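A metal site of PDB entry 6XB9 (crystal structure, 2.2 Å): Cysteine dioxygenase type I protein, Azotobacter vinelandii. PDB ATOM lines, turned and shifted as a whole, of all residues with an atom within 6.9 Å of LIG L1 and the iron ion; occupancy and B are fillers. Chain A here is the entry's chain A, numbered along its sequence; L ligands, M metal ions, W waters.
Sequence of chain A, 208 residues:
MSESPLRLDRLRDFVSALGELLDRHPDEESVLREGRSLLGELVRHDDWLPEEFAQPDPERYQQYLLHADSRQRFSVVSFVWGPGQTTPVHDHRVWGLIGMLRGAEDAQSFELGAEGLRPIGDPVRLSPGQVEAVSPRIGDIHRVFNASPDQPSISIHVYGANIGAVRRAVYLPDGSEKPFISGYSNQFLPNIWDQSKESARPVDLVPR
Within 4 Å of the iron ion: His 90, His 92 and His 142.
Residues that only touch LIG L1: Phe 79, Thr 87, Val 144 and His 157.
Within 4 Å of LIG L1: Phe 79, Thr 87, His 90, His 92, His 142, Val 144, His 157, Tyr 159 and Arg 168.
Along chain A the residues within 4 Å of LIG L1 span positions 79 to 168.
The nearest printed residue that does not touch LIG L1 is Phe 180 (4.5 Å).
The guanidinium group (NH2) of Arg 168 lies within salt-bridge range of an oxygen (O1) of LIG L1.
The side-chain hydroxyl (OH) of Tyr 159 lies close to an oxygen (O2) of LIG L1 (2.9 Å).
The iron ion is bound by a ring nitrogen (NE2) of His 90 (2.1 Å).
NE2 of His 142 is bound to the iron ion, 2.2 Å away.
O3 of LIG L1 binds the iron ion.
An oxygen (O2) of LIG L1 binds the iron ion, at 2.2 Å.
The iron ion is bound by NE2 of His 92, at 2.2 Å.
CL1 of LG2 L2 is bound to the iron ion (2.4 Å).
The iron ion has six donor atoms within binding distance.
The backbone carbonyl oxygen (O) of Pro 88 lies within hydrogen-bond range of a ring nitrogen (ND1) of His 90, 2.8 Å away.
The backbone carbonyl oxygen (O) of Arg 168 lies within hydrogen-bond range of the backbone NH (N) of Phe 180, at 2.7 Å.
The side-chain hydroxyl (OG) of Ser 182 is in hydrogen-bond range of the guanidinium group (NH2) of Arg 168.
OH of Tyr 159 lies within hydrogen-bond range of ND1 of His 157 (2.9 Å).
The backbone carbonyl oxygen (O) of Val 144 sits at hydrogen-bond distance from the backbone NH (N) of Thr 87 (3.0 Å).
The backbone carbonyl oxygen (O) of Val 144 is in hydrogen-bond range of the indole nitrogen (NE1) of Trp 81 (3.5 Å).
NE2 of His 157 lies within hydrogen-bond range of OG of Ser 155, 2.7 Å away.
The backbone NH (N) of Phe 79 lies within hydrogen-bond range of the backbone carbonyl oxygen (O) of Ser 155, 3.0 Å away.
Water W1 lies within hydrogen-bond range of the side-chain amide oxygen of Gln 63 (2.6 Å), the side-chain hydroxyl of Tyr 61 (2.6 Å) and an oxygen (O1) of LIG L1 (2.8 Å).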
ATOM      1  N   TYR A  61      35.029  29.147   4.777  1.00  0.00           N
ATOM      2  CA  TYR A  61      33.578  28.963   5.013  1.00  0.00           C
ATOM      3  C   TYR A  61      33.404  27.675   5.815  1.00  0.00           C
ATOM      4  O   TYR A  61      34.230  26.778   5.683  1.00  0.00           O
ATOM      5  CB  TYR A  61      32.823  28.969   3.675  1.00  0.00           C
ATOM      6  CG  TYR A  61      33.002  27.743   2.804  1.00  0.00           C
ATOM      7  CD1 TYR A  61      32.080  26.713   2.850  1.00  0.00           C
ATOM      8  CD2 TYR A  61      34.076  27.611   1.936  1.00  0.00           C
ATOM      9  CE1 TYR A  61      32.223  25.583   2.062  1.00  0.00           C
ATOM     10  CE2 TYR A  61      34.247  26.483   1.159  1.00  0.00           C
ATOM     11  CZ  TYR A  61      33.291  25.477   1.202  1.00  0.00           C
ATOM     12  OH  TYR A  61      33.419  24.363   0.423  1.00  0.00           O
ATOM     13  N   GLN A  63      31.132  24.345   7.391  1.00  0.00           N
ATOM     14  CA  GLN A  63      30.237  23.268   6.896  1.00  0.00           C
ATOM     15  C   GLN A  63      29.802  22.448   8.116  1.00  0.00           C
ATOM     16  O   GLN A  63      30.508  21.486   8.464  1.00  0.00           O
ATOM     17  CB  GLN A  63      30.983  22.391   5.888  1.00  0.00           C
ATOM     18  CG  GLN A  63      31.976  23.165   5.032  1.00  0.00           C
ATOM     19  CD  GLN A  63      32.557  22.340   3.895  1.00  0.00           C
ATOM     20  OE1 GLN A  63      31.892  21.496   3.301  1.00  0.00           O
ATOM     21  NE2 GLN A  63      33.818  22.585   3.584  1.00  0.00           N
ATOM     22  N   PHE A  79      25.730  25.881   6.067  1.00  0.00           N
ATOM     23  CA  PHE A  79      26.929  26.507   5.453  1.00  0.00           C
ATOM     24  C   PHE A  79      26.971  27.973   5.901  1.00  0.00           C
ATOM     25  O   PHE A  79      25.956  28.662   5.804  1.00  0.00           O
ATOM     26  CB  PHE A  79      26.924  26.361   3.937  1.00  0.00           C
ATOM     27  CG  PHE A  79      27.300  24.988   3.453  1.00  0.00           C
ATOM     28  CD1 PHE A  79      28.628  24.630   3.288  1.00  0.00           C
ATOM     29  CD2 PHE A  79      26.321  24.054   3.149  1.00  0.00           C
ATOM     30  CE1 PHE A  79      28.964  23.373   2.839  1.00  0.00           C
ATOM     31  CE2 PHE A  79      26.675  22.797   2.687  1.00  0.00           C
ATOM     32  CZ  PHE A  79      27.989  22.445   2.541  1.00  0.00           C
ATOM     33  N   TRP A  81      29.273  31.409   5.372  1.00  0.00           N
ATOM     34  CA  TRP A  81      30.308  32.258   4.738  1.00  0.00           C
ATOM     35  C   TRP A  81      30.479  33.525   5.576  1.00  0.00           C
ATOM     36  O   TRP A  81      29.461  34.125   5.935  1.00  0.00           O
ATOM     37  CB  TRP A  81      29.940  32.590   3.295  1.00  0.00           C
ATOM     38  CG  TRP A  81      29.921  31.415   2.379  1.00  0.00           C
ATOM     39  CD1 TRP A  81      30.924  30.992   1.578  1.00  0.00           C
ATOM     40  CD2 TRP A  81      28.836  30.487   2.183  1.00  0.00           C
ATOM     41  NE1 TRP A  81      30.546  29.870   0.871  1.00  0.00           N
ATOM     42  CE2 TRP A  81      29.264  29.548   1.226  1.00  0.00           C
ATOM     43  CE3 TRP A  81      27.536  30.380   2.708  1.00  0.00           C
ATOM     44  CZ2 TRP A  81      28.458  28.485   0.812  1.00  0.00           C
ATOM     45  CZ3 TRP A  81      26.737  29.351   2.288  1.00  0.00           C
ATOM     46  CH2 TRP A  81      27.186  28.420   1.339  1.00  0.00           C
ATOM     47  N   THR A  87      32.995  29.381  -1.856  1.00  0.00           N
ATOM     48  CA  THR A  87      33.363  27.968  -2.143  1.00  0.00           C
ATOM     49  C   THR A  87      34.318  27.969  -3.327  1.00  0.00           C
ATOM     50  O   THR A  87      34.383  28.944  -4.061  1.00  0.00           O
ATOM     51  CB  THR A  87      32.134  27.109  -2.483  1.00  0.00           C
ATOM     52  OG1 THR A  87      31.668  27.505  -3.756  1.00  0.00           O
ATOM     53  CG2 THR A  87      31.008  27.225  -1.472  1.00  0.00           C
ATOM     54  N   PRO A  88      35.073  26.884  -3.552  1.00  0.00           N
ATOM     55  CA  PRO A  88      35.662  26.652  -4.873  1.00  0.00           C
ATOM     56  C   PRO A  88      34.532  26.338  -5.872  1.00  0.00           C
ATOM     57  O   PRO A  88      33.389  26.140  -5.467  1.00  0.00           O
ATOM     58  CB  PRO A  88      36.599  25.461  -4.634  1.00  0.00           C
ATOM     59  CG  PRO A  88      35.989  24.730  -3.450  1.00  0.00           C
ATOM     60  CD  PRO A  88      35.414  25.837  -2.593  1.00  0.00           C
ATOM     61  N   HIS A  90      32.814  23.652  -7.760  1.00  0.00           N
ATOM     62  CA  HIS A  90      32.669  22.245  -7.337  1.00  0.00           C
ATOM     63  C   HIS A  90      31.395  21.649  -7.951  1.00  0.00           C
ATOM     64  O   HIS A  90      30.535  22.417  -8.381  1.00  0.00           O
ATOM     65  CB  HIS A  90      32.668  22.174  -5.804  1.00  0.00           C
ATOM     66  CG  HIS A  90      31.494  22.844  -5.182  1.00  0.00           C
ATOM     67  ND1 HIS A  90      31.493  24.182  -4.858  1.00  0.00           N
ATOM     68  CD2 HIS A  90      30.281  22.366  -4.843  1.00  0.00           C
ATOM     69  CE1 HIS A  90      30.319  24.505  -4.358  1.00  0.00           C
ATOM     70  NE2 HIS A  90      29.556  23.411  -4.321  1.00  0.00           N
ATOM     71  N   ASP A  91      31.346  20.311  -8.012  1.00  0.00           N
ATOM     72  CA  ASP A  91      30.122  19.528  -8.353  1.00  0.00           C
ATOM     73  C   ASP A  91      29.650  18.824  -7.069  1.00  0.00           C
ATOM     74  O   ASP A  91      30.188  19.149  -5.993  1.00  0.00           O
ATOM     75  CB  ASP A  91      30.397  18.580  -9.527  1.00  0.00           C
ATOM     76  CG  ASP A  91      31.469  17.530  -9.219  1.00  0.00           C
ATOM     77  OD1 ASP A  91      32.039  17.566  -8.113  1.00  0.00           O
ATOM     78  OD2 ASP A  91      31.731  16.689 -10.089  1.00  0.00           O
ATOM     79  N   HIS A  92      28.668  17.927  -7.177  1.00  0.00           N
ATOM     80  CA  HIS A  92      27.988  17.279  -6.013  1.00  0.00           C
ATOM     81  C   HIS A  92      27.869  15.777  -6.223  1.00  0.00           C
ATOM     82  O   HIS A  92      28.107  15.033  -5.264  1.00  0.00           O
ATOM     83  CB  HIS A  92      26.632  17.969  -5.771  1.00  0.00           C
ATOM     84  CG  HIS A  92      26.777  19.441  -5.594  1.00  0.00           C
ATOM     85  ND1 HIS A  92      26.776  20.308  -6.658  1.00  0.00           N
ATOM     86  CD2 HIS A  92      26.966  20.175  -4.479  1.00  0.00           C
ATOM     87  CE1 HIS A  92      26.945  21.537  -6.214  1.00  0.00           C
ATOM     88  NE2 HIS A  92      27.085  21.478  -4.876  1.00  0.00           N
ATOM     89  N   ILE A  98      19.412  24.061  -1.839  1.00  0.00           N
ATOM     90  CA  ILE A  98      20.053  25.195  -1.128  1.00  0.00           C
ATOM     91  C   ILE A  98      18.929  26.112  -0.640  1.00  0.00           C
ATOM     92  O   ILE A  98      18.280  26.710  -1.485  1.00  0.00           O
ATOM     93  CB  ILE A  98      21.013  25.958  -2.045  1.00  0.00           C
ATOM     94  CG1 ILE A  98      22.050  25.029  -2.695  1.00  0.00           C
ATOM     95  CG2 ILE A  98      21.659  27.119  -1.317  1.00  0.00           C
ATOM     96  CD1 ILE A  98      21.640  24.489  -4.043  1.00  0.00           C
ATOM     97  N   VAL A 134      20.494  21.586  -7.287  1.00  0.00           N
ATOM     98  CA  VAL A 134      21.618  21.105  -8.139  1.00  0.00           C
ATOM     99  C   VAL A 134      21.477  19.581  -8.267  1.00  0.00           C
ATOM    100  O   VAL A 134      20.807  18.982  -7.405  1.00  0.00           O
ATOM    101  CB  VAL A 134      22.996  21.506  -7.585  1.00  0.00           C
ATOM    102  CG1 VAL A 134      23.157  23.020  -7.584  1.00  0.00           C
ATOM    103  CG2 VAL A 134      23.262  20.938  -6.200  1.00  0.00           C
ATOM    104  N   ASP A 140      25.137  20.612 -12.136  1.00  0.00           N
ATOM    105  CA  ASP A 140      25.808  20.141 -10.906  1.00  0.00           C
ATOM    106  C   ASP A 140      26.952  21.084 -10.501  1.00  0.00           C
ATOM    107  O   ASP A 140      27.299  21.074  -9.313  1.00  0.00           O
ATOM    108  CB  ASP A 140      26.340  18.718 -11.103  1.00  0.00           C
ATOM    109  CG  ASP A 140      26.355  17.913  -9.818  1.00  0.00           C
ATOM    110  OD1 ASP A 140      25.474  18.171  -8.965  1.00  0.00           O
ATOM    111  OD2 ASP A 140      27.259  17.049  -9.661  1.00  0.00           O
ATOM    112  N   HIS A 142      28.819  24.571  -9.708  1.00  0.00           N
ATOM    113  CA  HIS A 142      28.539  25.963  -9.273  1.00  0.00           C
ATOM    114  C   HIS A 142      29.607  26.443  -8.289  1.00  0.00           C
ATOM    115  O   HIS A 142      30.480  25.649  -7.889  1.00  0.00           O
ATOM    116  CB  HIS A 142      27.108  26.076  -8.741  1.00  0.00           C
ATOM    117  CG  HIS A 142      26.868  25.493  -7.385  1.00  0.00           C
ATOM    118  ND1 HIS A 142      25.695  25.727  -6.691  1.00  0.00           N
ATOM    119  CD2 HIS A 142      27.608  24.694  -6.586  1.00  0.00           C
ATOM    120  CE1 HIS A 142      25.728  25.110  -5.539  1.00  0.00           C
ATOM    121  NE2 HIS A 142      26.885  24.458  -5.444  1.00  0.00           N
ATOM    122  N   ARG A 143      29.538  27.729  -7.963  1.00  0.00           N
ATOM    123  CA  ARG A 143      30.311  28.412  -6.896  1.00  0.00           C
ATOM    124  C   ARG A 143      29.316  29.266  -6.121  1.00  0.00           C
ATOM    125  O   ARG A 143      28.618  30.043  -6.771  1.00  0.00           O
ATOM    126  CB  ARG A 143      31.422  29.254  -7.510  1.00  0.00           C
ATOM    127  CG  ARG A 143      32.257  30.031  -6.513  1.00  0.00           C
ATOM    128  CD  ARG A 143      33.440  30.690  -7.194  1.00  0.00           C
ATOM    129  NE  ARG A 143      33.054  31.917  -7.884  1.00  0.00           N
ATOM    130  CZ  ARG A 143      32.905  33.100  -7.299  1.00  0.00           C
ATOM    131  NH1 ARG A 143      33.103  33.244  -5.997  1.00  0.00           N
ATOM    132  NH2 ARG A 143      32.545  34.143  -8.011  1.00  0.00           N
ATOM    133  N   VAL A 144      29.260  29.112  -4.797  1.00  0.00           N
ATOM    134  CA  VAL A 144      28.375  29.892  -3.882  1.00  0.00           C
ATOM    135  C   VAL A 144      29.247  30.833  -3.054  1.00  0.00           C
ATOM    136  O   VAL A 144      30.291  30.379  -2.572  1.00  0.00           O
ATOM    137  CB  VAL A 144      27.534  28.960  -3.000  1.00  0.00           C
ATOM    138  CG1 VAL A 144      26.570  29.719  -2.091  1.00  0.00           C
ATOM    139  CG2 VAL A 144      26.756  27.961  -3.846  1.00  0.00           C
ATOM    140  N   SER A 155      23.084  29.478   4.542  1.00  0.00           N
ATOM    141  CA  SER A 155      22.071  28.691   3.808  1.00  0.00           C
ATOM    142  C   SER A 155      22.075  27.260   4.358  1.00  0.00           C
ATOM    143  O   SER A 155      23.147  26.773   4.792  1.00  0.00           O
ATOM    144  CB  SER A 155      22.331  28.731   2.324  1.00  0.00           C
ATOM    145  OG  SER A 155      23.710  28.568   2.044  1.00  0.00           O
ATOM    146  N   HIS A 157      21.573  23.427   3.380  1.00  0.00           N
ATOM    147  CA  HIS A 157      21.689  22.571   2.173  1.00  0.00           C
ATOM    148  C   HIS A 157      21.270  21.150   2.539  1.00  0.00           C
ATOM    149  O   HIS A 157      21.563  20.709   3.674  1.00  0.00           O
ATOM    150  CB  HIS A 157      23.102  22.627   1.594  1.00  0.00           C
ATOM    151  CG  HIS A 157      23.560  23.985   1.188  1.00  0.00           C
ATOM    152  ND1 HIS A 157      24.432  24.184   0.141  1.00  0.00           N
ATOM    153  CD2 HIS A 157      23.306  25.210   1.692  1.00  0.00           C
ATOM    154  CE1 HIS A 157      24.692  25.461   0.017  1.00  0.00           C
ATOM    155  NE2 HIS A 157      24.013  26.118   0.950  1.00  0.00           N
ATOM    156  N   TYR A 159      21.254  17.134   0.704  1.00  0.00           N
ATOM    157  CA  TYR A 159      21.871  16.337  -0.376  1.00  0.00           C
ATOM    158  C   TYR A 159      21.378  14.900  -0.300  1.00  0.00           C
ATOM    159  O   TYR A 159      20.955  14.470   0.808  1.00  0.00           O
ATOM    160  CB  TYR A 159      23.397  16.388  -0.251  1.00  0.00           C
ATOM    161  CG  TYR A 159      23.969  17.772  -0.326  1.00  0.00           C
ATOM    162  CD1 TYR A 159      24.225  18.390  -1.541  1.00  0.00           C
ATOM    163  CD2 TYR A 159      24.227  18.489   0.839  1.00  0.00           C
ATOM    164  CE1 TYR A 159      24.745  19.666  -1.614  1.00  0.00           C
ATOM    165  CE2 TYR A 159      24.750  19.774   0.786  1.00  0.00           C
ATOM    166  CZ  TYR A 159      25.017  20.359  -0.435  1.00  0.00           C
ATOM    167  OH  TYR A 159      25.525  21.628  -0.494  1.00  0.00           O
ATOM    168  N   ILE A 163      27.153  14.177   2.344  1.00  0.00           N
ATOM    169  CA  ILE A 163      27.876  15.040   1.345  1.00  0.00           C
ATOM    170  C   ILE A 163      29.336  15.200   1.757  1.00  0.00           C
ATOM    171  O   ILE A 163      30.206  15.257   0.849  1.00  0.00           O
ATOM    172  CB  ILE A 163      27.174  16.399   1.174  1.00  0.00           C
ATOM    173  CG1 ILE A 163      27.711  17.185  -0.017  1.00  0.00           C
ATOM    174  CG2 ILE A 163      27.236  17.238   2.454  1.00  0.00           C
ATOM    175  CD1 ILE A 163      27.509  16.489  -1.361  1.00  0.00           C
ATOM    176  N   ARG A 168      33.931  13.836  -4.896  1.00  0.00           N
ATOM    177  CA  ARG A 168      33.505  14.737  -5.996  1.00  0.00           C
ATOM    178  C   ARG A 168      34.737  15.557  -6.435  1.00  0.00           C
ATOM    179  O   ARG A 168      35.867  15.123  -6.136  1.00  0.00           O
ATOM    180  CB  ARG A 168      32.315  15.576  -5.544  1.00  0.00           C
ATOM    181  CG  ARG A 168      32.361  16.024  -4.102  1.00  0.00           C
ATOM    182  CD  ARG A 168      31.142  16.854  -3.761  1.00  0.00           C
ATOM    183  NE  ARG A 168      31.207  17.427  -2.424  1.00  0.00           N
ATOM    184  CZ  ARG A 168      30.668  18.582  -2.068  1.00  0.00           C
ATOM    185  NH1 ARG A 168      30.035  19.325  -2.957  1.00  0.00           N
ATOM    186  NH2 ARG A 168      30.776  19.021  -0.827  1.00  0.00           N
ATOM    187  N   PHE A 180      37.804  15.982  -4.481  1.00  0.00           N
ATOM    188  CA  PHE A 180      37.172  16.824  -3.435  1.00  0.00           C
ATOM    189  C   PHE A 180      36.326  15.941  -2.521  1.00  0.00           C
ATOM    190  O   PHE A 180      35.389  15.278  -2.994  1.00  0.00           O
ATOM    191  CB  PHE A 180      36.345  17.941  -4.074  1.00  0.00           C
ATOM    192  CG  PHE A 180      35.765  18.948  -3.115  1.00  0.00           C
ATOM    193  CD1 PHE A 180      36.522  19.461  -2.072  1.00  0.00           C
ATOM    194  CD2 PHE A 180      34.475  19.416  -3.283  1.00  0.00           C
ATOM    195  CE1 PHE A 180      35.998  20.451  -1.241  1.00  0.00           C
ATOM    196  CE2 PHE A 180      33.938  20.368  -2.438  1.00  0.00           C
ATOM    197  CZ  PHE A 180      34.709  20.886  -1.423  1.00  0.00           C
ATOM    198  N   SER A 182      34.696  17.096   1.138  1.00  0.00           N
ATOM    199  CA  SER A 182      34.523  18.376   1.860  1.00  0.00           C
ATOM    200  C   SER A 182      34.640  18.168   3.373  1.00  0.00           C
ATOM    201  O   SER A 182      35.177  19.060   4.049  1.00  0.00           O
ATOM    202  CB  SER A 182      33.217  19.031   1.489  1.00  0.00           C
ATOM    203  OG  SER A 182      32.143  18.098   1.537  1.00  0.00           O
HETATM  204  C1  LIG L   1      28.837  22.424  -1.462  1.00  0.00           C
HETATM  205  O1  LIG L   1      29.907  21.757  -1.128  1.00  0.00           O
HETATM  206  O2  LIG L   1      27.943  21.928  -2.112  1.00  0.00           O
HETATM  207  C2  LIG L   1      28.829  23.833  -0.957  1.00  0.00           C
HETATM  208  C3  LIG L   1      27.745  24.720  -1.574  1.00  0.00           C
HETATM  209  O3  LIG L   1      28.090  25.175  -2.887  1.00  0.00           O
HETATM  210 CL1  LG2 L   2      25.292  23.006  -2.954  1.00  0.00          CL
HETATM  211 FE    FE M   1      27.490  23.280  -3.742  1.00  0.00          FE
HETATM  212  O   HOH W   1      31.891  22.251   0.839  1.00  0.00           O
